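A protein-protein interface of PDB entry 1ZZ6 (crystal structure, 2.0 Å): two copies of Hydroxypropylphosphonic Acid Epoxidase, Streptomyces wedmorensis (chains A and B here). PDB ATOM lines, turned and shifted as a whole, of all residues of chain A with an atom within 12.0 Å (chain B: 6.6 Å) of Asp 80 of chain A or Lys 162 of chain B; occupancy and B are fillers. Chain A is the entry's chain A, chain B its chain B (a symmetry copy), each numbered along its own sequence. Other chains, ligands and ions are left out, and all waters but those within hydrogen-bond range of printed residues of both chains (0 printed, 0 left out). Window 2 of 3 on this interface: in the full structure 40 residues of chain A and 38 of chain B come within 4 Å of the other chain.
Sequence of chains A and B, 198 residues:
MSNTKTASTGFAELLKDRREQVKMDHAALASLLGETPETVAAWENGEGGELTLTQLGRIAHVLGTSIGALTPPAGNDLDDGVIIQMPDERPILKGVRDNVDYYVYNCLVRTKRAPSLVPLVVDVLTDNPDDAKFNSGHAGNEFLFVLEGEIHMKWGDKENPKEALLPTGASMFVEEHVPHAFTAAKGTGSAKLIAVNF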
ATOM      1  N   GLY A  75      -6.468  14.983 -25.311  1.00  0.00           N
ATOM      2  CA  GLY A  75      -6.921  13.607 -25.226  1.00  0.00           C
ATOM      3  C   GLY A  75      -5.888  12.738 -24.530  1.00  0.00           C
ATOM      4  O   GLY A  75      -4.842  13.238 -24.096  1.00  0.00           O
ATOM      5  N   ASN A  76      -6.165  11.438 -24.423  1.00  0.00           N
ATOM      6  CA  ASN A  76      -5.237  10.529 -23.755  1.00  0.00           C
ATOM      7  C   ASN A  76      -4.878   9.338 -24.631  1.00  0.00           C
ATOM      8  O   ASN A  76      -5.720   8.485 -24.905  1.00  0.00           O
ATOM      9  CB  ASN A  76      -5.840  10.026 -22.446  1.00  0.00           C
ATOM     10  CG  ASN A  76      -4.799   9.423 -21.527  1.00  0.00           C
ATOM     11  OD1 ASN A  76      -3.909   8.695 -21.971  1.00  0.00           O
ATOM     12  ND2 ASN A  76      -4.909   9.717 -20.238  1.00  0.00           N
ATOM     13  N   ASP A  77      -3.618   9.290 -25.059  1.00  0.00           N
ATOM     14  CA  ASP A  77      -3.128   8.220 -25.923  1.00  0.00           C
ATOM     15  C   ASP A  77      -2.139   7.317 -25.200  1.00  0.00           C
ATOM     16  O   ASP A  77      -1.365   6.596 -25.842  1.00  0.00           O
ATOM     17  CB  ASP A  77      -2.437   8.818 -27.153  1.00  0.00           C
ATOM     18  CG  ASP A  77      -1.404   9.874 -26.783  1.00  0.00           C
ATOM     19  OD1 ASP A  77      -1.055   9.984 -25.587  1.00  0.00           O
ATOM     20  OD2 ASP A  77      -0.941  10.596 -27.687  1.00  0.00           O
ATOM     21  N   LEU A  78      -2.156   7.371 -23.874  1.00  0.00           N
ATOM     22  CA  LEU A  78      -1.245   6.577 -23.063  1.00  0.00           C
ATOM     23  C   LEU A  78      -1.837   5.228 -22.691  1.00  0.00           C
ATOM     24  O   LEU A  78      -3.051   5.035 -22.738  1.00  0.00           O
ATOM     25  CB  LEU A  78      -0.884   7.338 -21.784  1.00  0.00           C
ATOM     26  CG  LEU A  78      -0.254   8.723 -21.979  1.00  0.00           C
ATOM     27  CD1 LEU A  78      -0.027   9.365 -20.624  1.00  0.00           C
ATOM     28  CD2 LEU A  78       1.061   8.597 -22.750  1.00  0.00           C
ATOM     29  N   ASP A  79      -0.959   4.298 -22.326  1.00  0.00           N
ATOM     30  CA  ASP A  79      -1.359   2.961 -21.912  1.00  0.00           C
ATOM     31  C   ASP A  79      -0.976   2.879 -20.443  1.00  0.00           C
ATOM     32  O   ASP A  79       0.156   2.535 -20.108  1.00  0.00           O
ATOM     33  CB  ASP A  79      -0.595   1.902 -22.705  1.00  0.00           C
ATOM     34  CG  ASP A  79      -1.203   0.521 -22.567  1.00  0.00           C
ATOM     35  OD1 ASP A  79      -1.520   0.114 -21.431  1.00  0.00           O
ATOM     36  OD2 ASP A  79      -1.361  -0.162 -23.596  1.00  0.00           O
ATOM     37  N   ASP A  80      -1.923   3.198 -19.567  1.00  0.00           N
ATOM     38  CA  ASP A  80      -1.654   3.194 -18.139  1.00  0.00           C
ATOM     39  C   ASP A  80      -0.464   4.104 -17.864  1.00  0.00           C
ATOM     40  O   ASP A  80       0.469   3.746 -17.143  1.00  0.00           O
ATOM     41  CB  ASP A  80      -1.374   1.775 -17.638  1.00  0.00           C
ATOM     42  CG  ASP A  80      -2.645   0.957 -17.470  1.00  0.00           C
ATOM     43  OD1 ASP A  80      -3.556   1.423 -16.755  1.00  0.00           O
ATOM     44  OD2 ASP A  80      -2.740  -0.148 -18.044  1.00  0.00           O
ATOM     45  N   GLY A  81      -0.508   5.287 -18.469  1.00  0.00           N
ATOM     46  CA  GLY A  81       0.540   6.268 -18.278  1.00  0.00           C
ATOM     47  C   GLY A  81       1.762   6.153 -19.170  1.00  0.00           C
ATOM     48  O   GLY A  81       2.660   6.986 -19.088  1.00  0.00           O
ATOM     49  N   VAL A  82       1.803   5.146 -20.034  1.00  0.00           N
ATOM     50  CA  VAL A  82       2.956   4.969 -20.904  1.00  0.00           C
ATOM     51  C   VAL A  82       2.622   4.886 -22.389  1.00  0.00           C
ATOM     52  O   VAL A  82       1.555   4.422 -22.782  1.00  0.00           O
ATOM     53  CB  VAL A  82       3.749   3.688 -20.506  1.00  0.00           C
ATOM     54  CG1 VAL A  82       4.833   3.397 -21.533  1.00  0.00           C
ATOM     55  CG2 VAL A  82       4.380   3.866 -19.139  1.00  0.00           C
ATOM     56  N   ILE A  83       3.547   5.370 -23.210  1.00  0.00           N
ATOM     57  CA  ILE A  83       3.415   5.302 -24.663  1.00  0.00           C
ATOM     58  C   ILE A  83       4.825   4.969 -25.131  1.00  0.00           C
ATOM     59  O   ILE A  83       5.805   5.541 -24.639  1.00  0.00           O
ATOM     60  CB  ILE A  83       2.911   6.630 -25.279  1.00  0.00           C
ATOM     61  CG1 ILE A  83       2.602   6.417 -26.761  1.00  0.00           C
ATOM     62  CG2 ILE A  83       3.933   7.735 -25.078  1.00  0.00           C
ATOM     63  CD1 ILE A  83       1.983   7.637 -27.453  1.00  0.00           C
ATOM     64  N   ILE A  84       4.926   4.021 -26.054  1.00  0.00           N
ATOM     65  CA  ILE A  84       6.216   3.569 -26.550  1.00  0.00           C
ATOM     66  C   ILE A  84       6.309   3.632 -28.060  1.00  0.00           C
ATOM     67  O   ILE A  84       5.327   3.396 -28.758  1.00  0.00           O
ATOM     68  CB  ILE A  84       6.477   2.108 -26.129  1.00  0.00           C
ATOM     69  CG1 ILE A  84       6.541   2.015 -24.606  1.00  0.00           C
ATOM     70  CG2 ILE A  84       7.761   1.594 -26.773  1.00  0.00           C
ATOM     71  CD1 ILE A  84       6.697   0.610 -24.084  1.00  0.00           C
ATOM     72  N   THR A 111       3.326  12.692 -27.366  1.00  0.00           N
ATOM     73  CA  THR A 111       2.073  12.358 -26.695  1.00  0.00           C
ATOM     74  C   THR A 111       1.148  13.541 -26.501  1.00  0.00           C
ATOM     75  O   THR A 111       1.600  14.648 -26.191  1.00  0.00           O
ATOM     76  CB  THR A 111       2.298  11.728 -25.305  1.00  0.00           C
ATOM     77  OG1 THR A 111       1.031  11.597 -24.643  1.00  0.00           O
ATOM     78  CG2 THR A 111       3.198  12.600 -24.451  1.00  0.00           C
ATOM     79  N   ARG A 113      -0.649  14.029 -24.130  1.00  0.00           N
ATOM     80  CA  ARG A 113      -0.700  14.389 -22.712  1.00  0.00           C
ATOM     81  C   ARG A 113       0.422  15.374 -22.341  1.00  0.00           C
ATOM     82  O   ARG A 113       0.472  15.882 -21.220  1.00  0.00           O
ATOM     83  CB  ARG A 113      -0.605  13.131 -21.852  1.00  0.00           C
ATOM     84  CG  ARG A 113      -1.814  12.203 -21.992  1.00  0.00           C
ATOM     85  CD  ARG A 113      -3.013  12.678 -21.170  1.00  0.00           C
ATOM     86  NE  ARG A 113      -2.849  12.358 -19.756  1.00  0.00           N
ATOM     87  CZ  ARG A 113      -3.776  12.563 -18.821  1.00  0.00           C
ATOM     88  NH1 ARG A 113      -4.948  13.095 -19.144  1.00  0.00           N
ATOM     89  NH2 ARG A 113      -3.535  12.220 -17.561  1.00  0.00           N
ATOM     90  N   PHE B 134       9.968  -1.147  -8.511  1.00  0.00           N
ATOM     91  CA  PHE B 134       9.245   0.031  -8.970  1.00  0.00           C
ATOM     92  C   PHE B 134       9.653   1.292  -8.212  1.00  0.00           C
ATOM     93  O   PHE B 134       9.811   1.271  -6.992  1.00  0.00           O
ATOM     94  CB  PHE B 134       7.737  -0.194  -8.828  1.00  0.00           C
ATOM     95  CG  PHE B 134       7.176  -1.173  -9.822  1.00  0.00           C
ATOM     96  CD1 PHE B 134       7.744  -2.435  -9.975  1.00  0.00           C
ATOM     97  CD2 PHE B 134       6.079  -0.833 -10.605  1.00  0.00           C
ATOM     98  CE1 PHE B 134       7.226  -3.342 -10.894  1.00  0.00           C
ATOM     99  CE2 PHE B 134       5.554  -1.735 -11.528  1.00  0.00           C
ATOM    100  CZ  PHE B 134       6.129  -2.991 -11.672  1.00  0.00           C
ATOM    101  N   MET B 153      11.092  -3.095 -19.555  1.00  0.00           N
ATOM    102  CA  MET B 153      10.345  -2.116 -18.771  1.00  0.00           C
ATOM    103  C   MET B 153       9.083  -2.705 -18.147  1.00  0.00           C
ATOM    104  O   MET B 153       8.364  -3.466 -18.787  1.00  0.00           O
ATOM    105  CB  MET B 153       9.972  -0.931 -19.673  1.00  0.00           C
ATOM    106  CG  MET B 153       9.351   0.267 -18.972  1.00  0.00           C
ATOM    107  SD  MET B 153       8.541   1.382 -20.168  1.00  0.00           S
ATOM    108  CE  MET B 153       9.729   2.704 -20.358  1.00  0.00           C
ATOM    109  N   LYS B 154       8.823  -2.336 -16.896  1.00  0.00           N
ATOM    110  CA  LYS B 154       7.642  -2.794 -16.172  1.00  0.00           C
ATOM    111  C   LYS B 154       6.979  -1.590 -15.504  1.00  0.00           C
ATOM    112  O   LYS B 154       7.665  -0.731 -14.950  1.00  0.00           O
ATOM    113  CB  LYS B 154       8.037  -3.836 -15.115  1.00  0.00           C
ATOM    114  CG  LYS B 154       8.736  -5.054 -15.705  1.00  0.00           C
ATOM    115  CD  LYS B 154       8.593  -6.301 -14.837  1.00  0.00           C
ATOM    116  CE  LYS B 154       9.308  -6.180 -13.503  1.00  0.00           C
ATOM    117  NZ  LYS B 154       9.140  -7.422 -12.684  1.00  0.00           N
ATOM    118  N   TRP B 155       5.652  -1.517 -15.561  1.00  0.00           N
ATOM    119  CA  TRP B 155       4.951  -0.388 -14.953  1.00  0.00           C
ATOM    120  C   TRP B 155       3.501  -0.705 -14.602  1.00  0.00           C
ATOM    121  O   TRP B 155       2.927  -1.673 -15.102  1.00  0.00           O
ATOM    122  CB  TRP B 155       5.004   0.827 -15.891  1.00  0.00           C
ATOM    123  CG  TRP B 155       4.055   0.771 -17.065  1.00  0.00           C
ATOM    124  CD1 TRP B 155       2.797   1.301 -17.128  1.00  0.00           C
ATOM    125  CD2 TRP B 155       4.304   0.182 -18.349  1.00  0.00           C
ATOM    126  NE1 TRP B 155       2.250   1.083 -18.370  1.00  0.00           N
ATOM    127  CE2 TRP B 155       3.153   0.398 -19.138  1.00  0.00           C
ATOM    128  CE3 TRP B 155       5.390  -0.506 -18.909  1.00  0.00           C
ATOM    129  CZ2 TRP B 155       3.055  -0.049 -20.460  1.00  0.00           C
ATOM    130  CZ3 TRP B 155       5.295  -0.950 -20.220  1.00  0.00           C
ATOM    131  CH2 TRP B 155       4.133  -0.719 -20.983  1.00  0.00           C
ATOM    132  N   GLY B 156       2.913   0.120 -13.742  1.00  0.00           N
ATOM    133  CA  GLY B 156       1.533  -0.094 -13.344  1.00  0.00           C
ATOM    134  C   GLY B 156       1.421  -0.737 -11.975  1.00  0.00           C
ATOM    135  O   GLY B 156       1.728  -0.107 -10.961  1.00  0.00           O
ATOM    136  N   ASP B 157       0.983  -1.992 -11.944  1.00  0.00           N
ATOM    137  CA  ASP B 157       0.832  -2.721 -10.687  1.00  0.00           C
ATOM    138  C   ASP B 157       2.086  -3.500 -10.311  1.00  0.00           C
ATOM    139  O   ASP B 157       2.451  -4.472 -10.977  1.00  0.00           O
ATOM    140  CB  ASP B 157      -0.359  -3.682 -10.768  1.00  0.00           C
ATOM    141  CG  ASP B 157      -1.693  -2.962 -10.743  1.00  0.00           C
ATOM    142  OD1 ASP B 157      -2.737  -3.646 -10.768  1.00  0.00           O
ATOM    143  OD2 ASP B 157      -1.698  -1.713 -10.696  1.00  0.00           O
ATOM    144  N   LYS B 162       2.144  -4.081 -16.185  1.00  0.00           N
ATOM    145  CA  LYS B 162       2.535  -4.350 -17.565  1.00  0.00           C
ATOM    146  C   LYS B 162       4.022  -4.229 -17.790  1.00  0.00           C
ATOM    147  O   LYS B 162       4.743  -3.630 -16.992  1.00  0.00           O
ATOM    148  CB  LYS B 162       1.831  -3.396 -18.520  1.00  0.00           C
ATOM    149  CG  LYS B 162       0.349  -3.691 -18.688  1.00  0.00           C
ATOM    150  CD  LYS B 162      -0.348  -2.498 -19.279  1.00  0.00           C
ATOM    151  CE  LYS B 162      -0.189  -1.318 -18.341  1.00  0.00           C
ATOM    152  NZ  LYS B 162      -0.777  -1.652 -17.000  1.00  0.00           N
ATOM    153  N   GLU B 163       4.471  -4.789 -18.905  1.00  0.00           N
ATOM    154  CA  GLU B 163       5.872  -4.753 -19.252  1.00  0.00           C
ATOM    155  C   GLU B 163       6.052  -4.731 -20.761  1.00  0.00           C
ATOM    156  O   GLU B 163       5.098  -4.907 -21.518  1.00  0.00           O
ATOM    157  CB  GLU B 163       6.591  -5.964 -18.654  1.00  0.00           C
ATOM    158  CG  GLU B 163       5.950  -7.294 -18.992  1.00  0.00           C
ATOM    159  CD  GLU B 163       6.767  -8.476 -18.507  1.00  0.00           C
ATOM    160  OE1 GLU B 163       7.047  -8.551 -17.289  1.00  0.00           O
ATOM    161  OE2 GLU B 163       7.128  -9.329 -19.347  1.00  0.00           O
ATOM    162  N   ALA B 164       7.283  -4.507 -21.192  1.00  0.00           N
ATOM    163  CA  ALA B 164       7.588  -4.459 -22.608  1.00  0.00           C
ATOM    164  C   ALA B 164       9.086  -4.540 -22.786  1.00  0.00           C
ATOM    165  O   ALA B 164       9.839  -4.074 -21.936  1.00  0.00           O
ATOM    166  CB  ALA B 164       7.063  -3.164 -23.211  1.00  0.00           C
ATOM    167  N   GLU B 175       4.196   9.074 -17.821  1.00  0.00           N
ATOM    168  CA  GLU B 175       3.517  10.181 -17.148  1.00  0.00           C
ATOM    169  C   GLU B 175       3.850  10.233 -15.661  1.00  0.00           C
ATOM    170  O   GLU B 175       4.290   9.248 -15.075  1.00  0.00           O
ATOM    171  CB  GLU B 175       2.006  10.052 -17.329  1.00  0.00           C
ATOM    172  CG  GLU B 175       1.268  11.357 -17.271  1.00  0.00           C
ATOM    173  CD  GLU B 175      -0.230  11.173 -17.428  1.00  0.00           C
ATOM    174  OE1 GLU B 175      -0.904  12.129 -17.864  1.00  0.00           O
ATOM    175  OE2 GLU B 175      -0.729  10.076 -17.105  1.00  0.00           O
ATOM    176  N   VAL B 178       3.524   7.596 -12.374  1.00  0.00           N
ATOM    177  CA  VAL B 178       3.445   6.240 -12.903  1.00  0.00           C
ATOM    178  C   VAL B 178       4.601   5.386 -12.394  1.00  0.00           C
ATOM    179  O   VAL B 178       5.739   5.537 -12.838  1.00  0.00           O
ATOM    180  CB  VAL B 178       3.468   6.236 -14.448  1.00  0.00           C
ATOM    181  CG1 VAL B 178       3.424   4.804 -14.967  1.00  0.00           C
ATOM    182  CG2 VAL B 178       2.293   7.029 -14.984  1.00  0.00           C
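The indole nitrogen (NE1) of Trp 155 of chain B sits at hydrogen-bond distance from the backbone carbonyl oxygen (O) of Asp 79 of chain A, 3.1 Å away.
The indole nitrogen (NE1) of Trp 155 of chain B sits close to the backbone carbonyl oxygen (O) of Asp 80 of chain A (3.4 Å).
The side-chain amino group (NZ) of Lys 162 of chain B lies within salt-bridge range of the side-chain carboxylate (OD2) of Asp 80 of chain A, at 2.7 Å.
OE1 of Glu 175 of chain B lies within salt-bridge range of NH2 of Arg 113 of chain A, at 2.6 Å.
The backbone carbonyl oxygen (O) of Gly 81 of chain A sits at hydrogen-bond distance from the backbone NH (N) of Glu 175 of chain B, 2.9 Å away.
The side-chain amide oxygen (OD1) of Asn 76 of chain A lies within hydrogen-bond range of the backbone NH (N) of Leu 78 of chain A (2.9 Å).
ND2 of Asn 76 of chain A lies close to NE of Arg 113 of chain A (3.4 Å).
The backbone carbonyl oxygen (O) of Lys 162 of chain B sits at hydrogen-bond distance from the backbone NH (N) of Trp 155 of chain B, 2.7 Å away.
The backbone NH of Ala 164 of chain B sits at hydrogen-bond distance from the backbone carbonyl oxygen of Met 153 of chain B.
The side-chain hydroxyl (OG1) of Thr 111 of chain A is in hydrogen-bond range of the backbone NH (N) of Arg 113 of chain A (3.0 Å).
Leu 78 of chain A touches Glu 175 of chain B (CD1 to OE2, 3.7 Å).
OD1 of Asp 79 of chain A touches CD of Lys 162 of chain B, at 3.6 Å.
O of Asp 80 of chain A touches CG1 of Val 178 of chain B (3.8 Å).
Gly 81 of chain A touches Val 178 of chain B (CA to CG2, 3.8 Å).
Val 82 of chain A touches Trp 155 of chain B (CG2 to NE1, 3.6 Å).
Ile 84 of chain A touches Ala 164 of chain B (CD1 to CB, 3.9 Å).
Asp 80 of chain A touches just these residues of chain B: Trp 155, Lys 162 and Val 178.
Of chain A, only Asp 79 and Asp 80 come within 4 Å of Lys 162 of chain B.
No residue of chain A comes within 4 Å of Lys 154 of chain B.
No residue of chain A comes within 4 Å of Gly 156 of chain B.
No residue of chain A comes within 4 Å of Asp 157 of chain B.
Val 178 of chain B touches just these residues of chain A: Asp 80 and Gly 81.
Of the printed residues of chain B, Val 82 of chain A touches Trp 155 (3.6 Å).
Printed residues of chain A within 4 Å of Glu 175 of chain B: Leu 78 (3.7 Å), Gly 81 (2.9 Å) and Arg 113 (2.6 Å).
Gly 75 of chain A touches none of the printed residues of chain B.
Asn 76 of chain A touches none of the printed residues of chain B.
The nearest residue of chain B that does not touch Asp 80 of chain A is Gly 156 of chain B (5.5 Å).
The nearest residue of chain A that does not touch Lys 162 of chain B is Gly 81 of chain A (6.6 Å).
The nearest printed residue of chain B that does not touch Ile 84 of chain A is Trp 155 of chain B (4.2 Å).
Of the 12 printed residues of chain A, 7 touch a printed residue of chain B.
Of the 11 printed residues of chain B, 5 touch a printed residue of chain A.
No position is printed for both chains.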
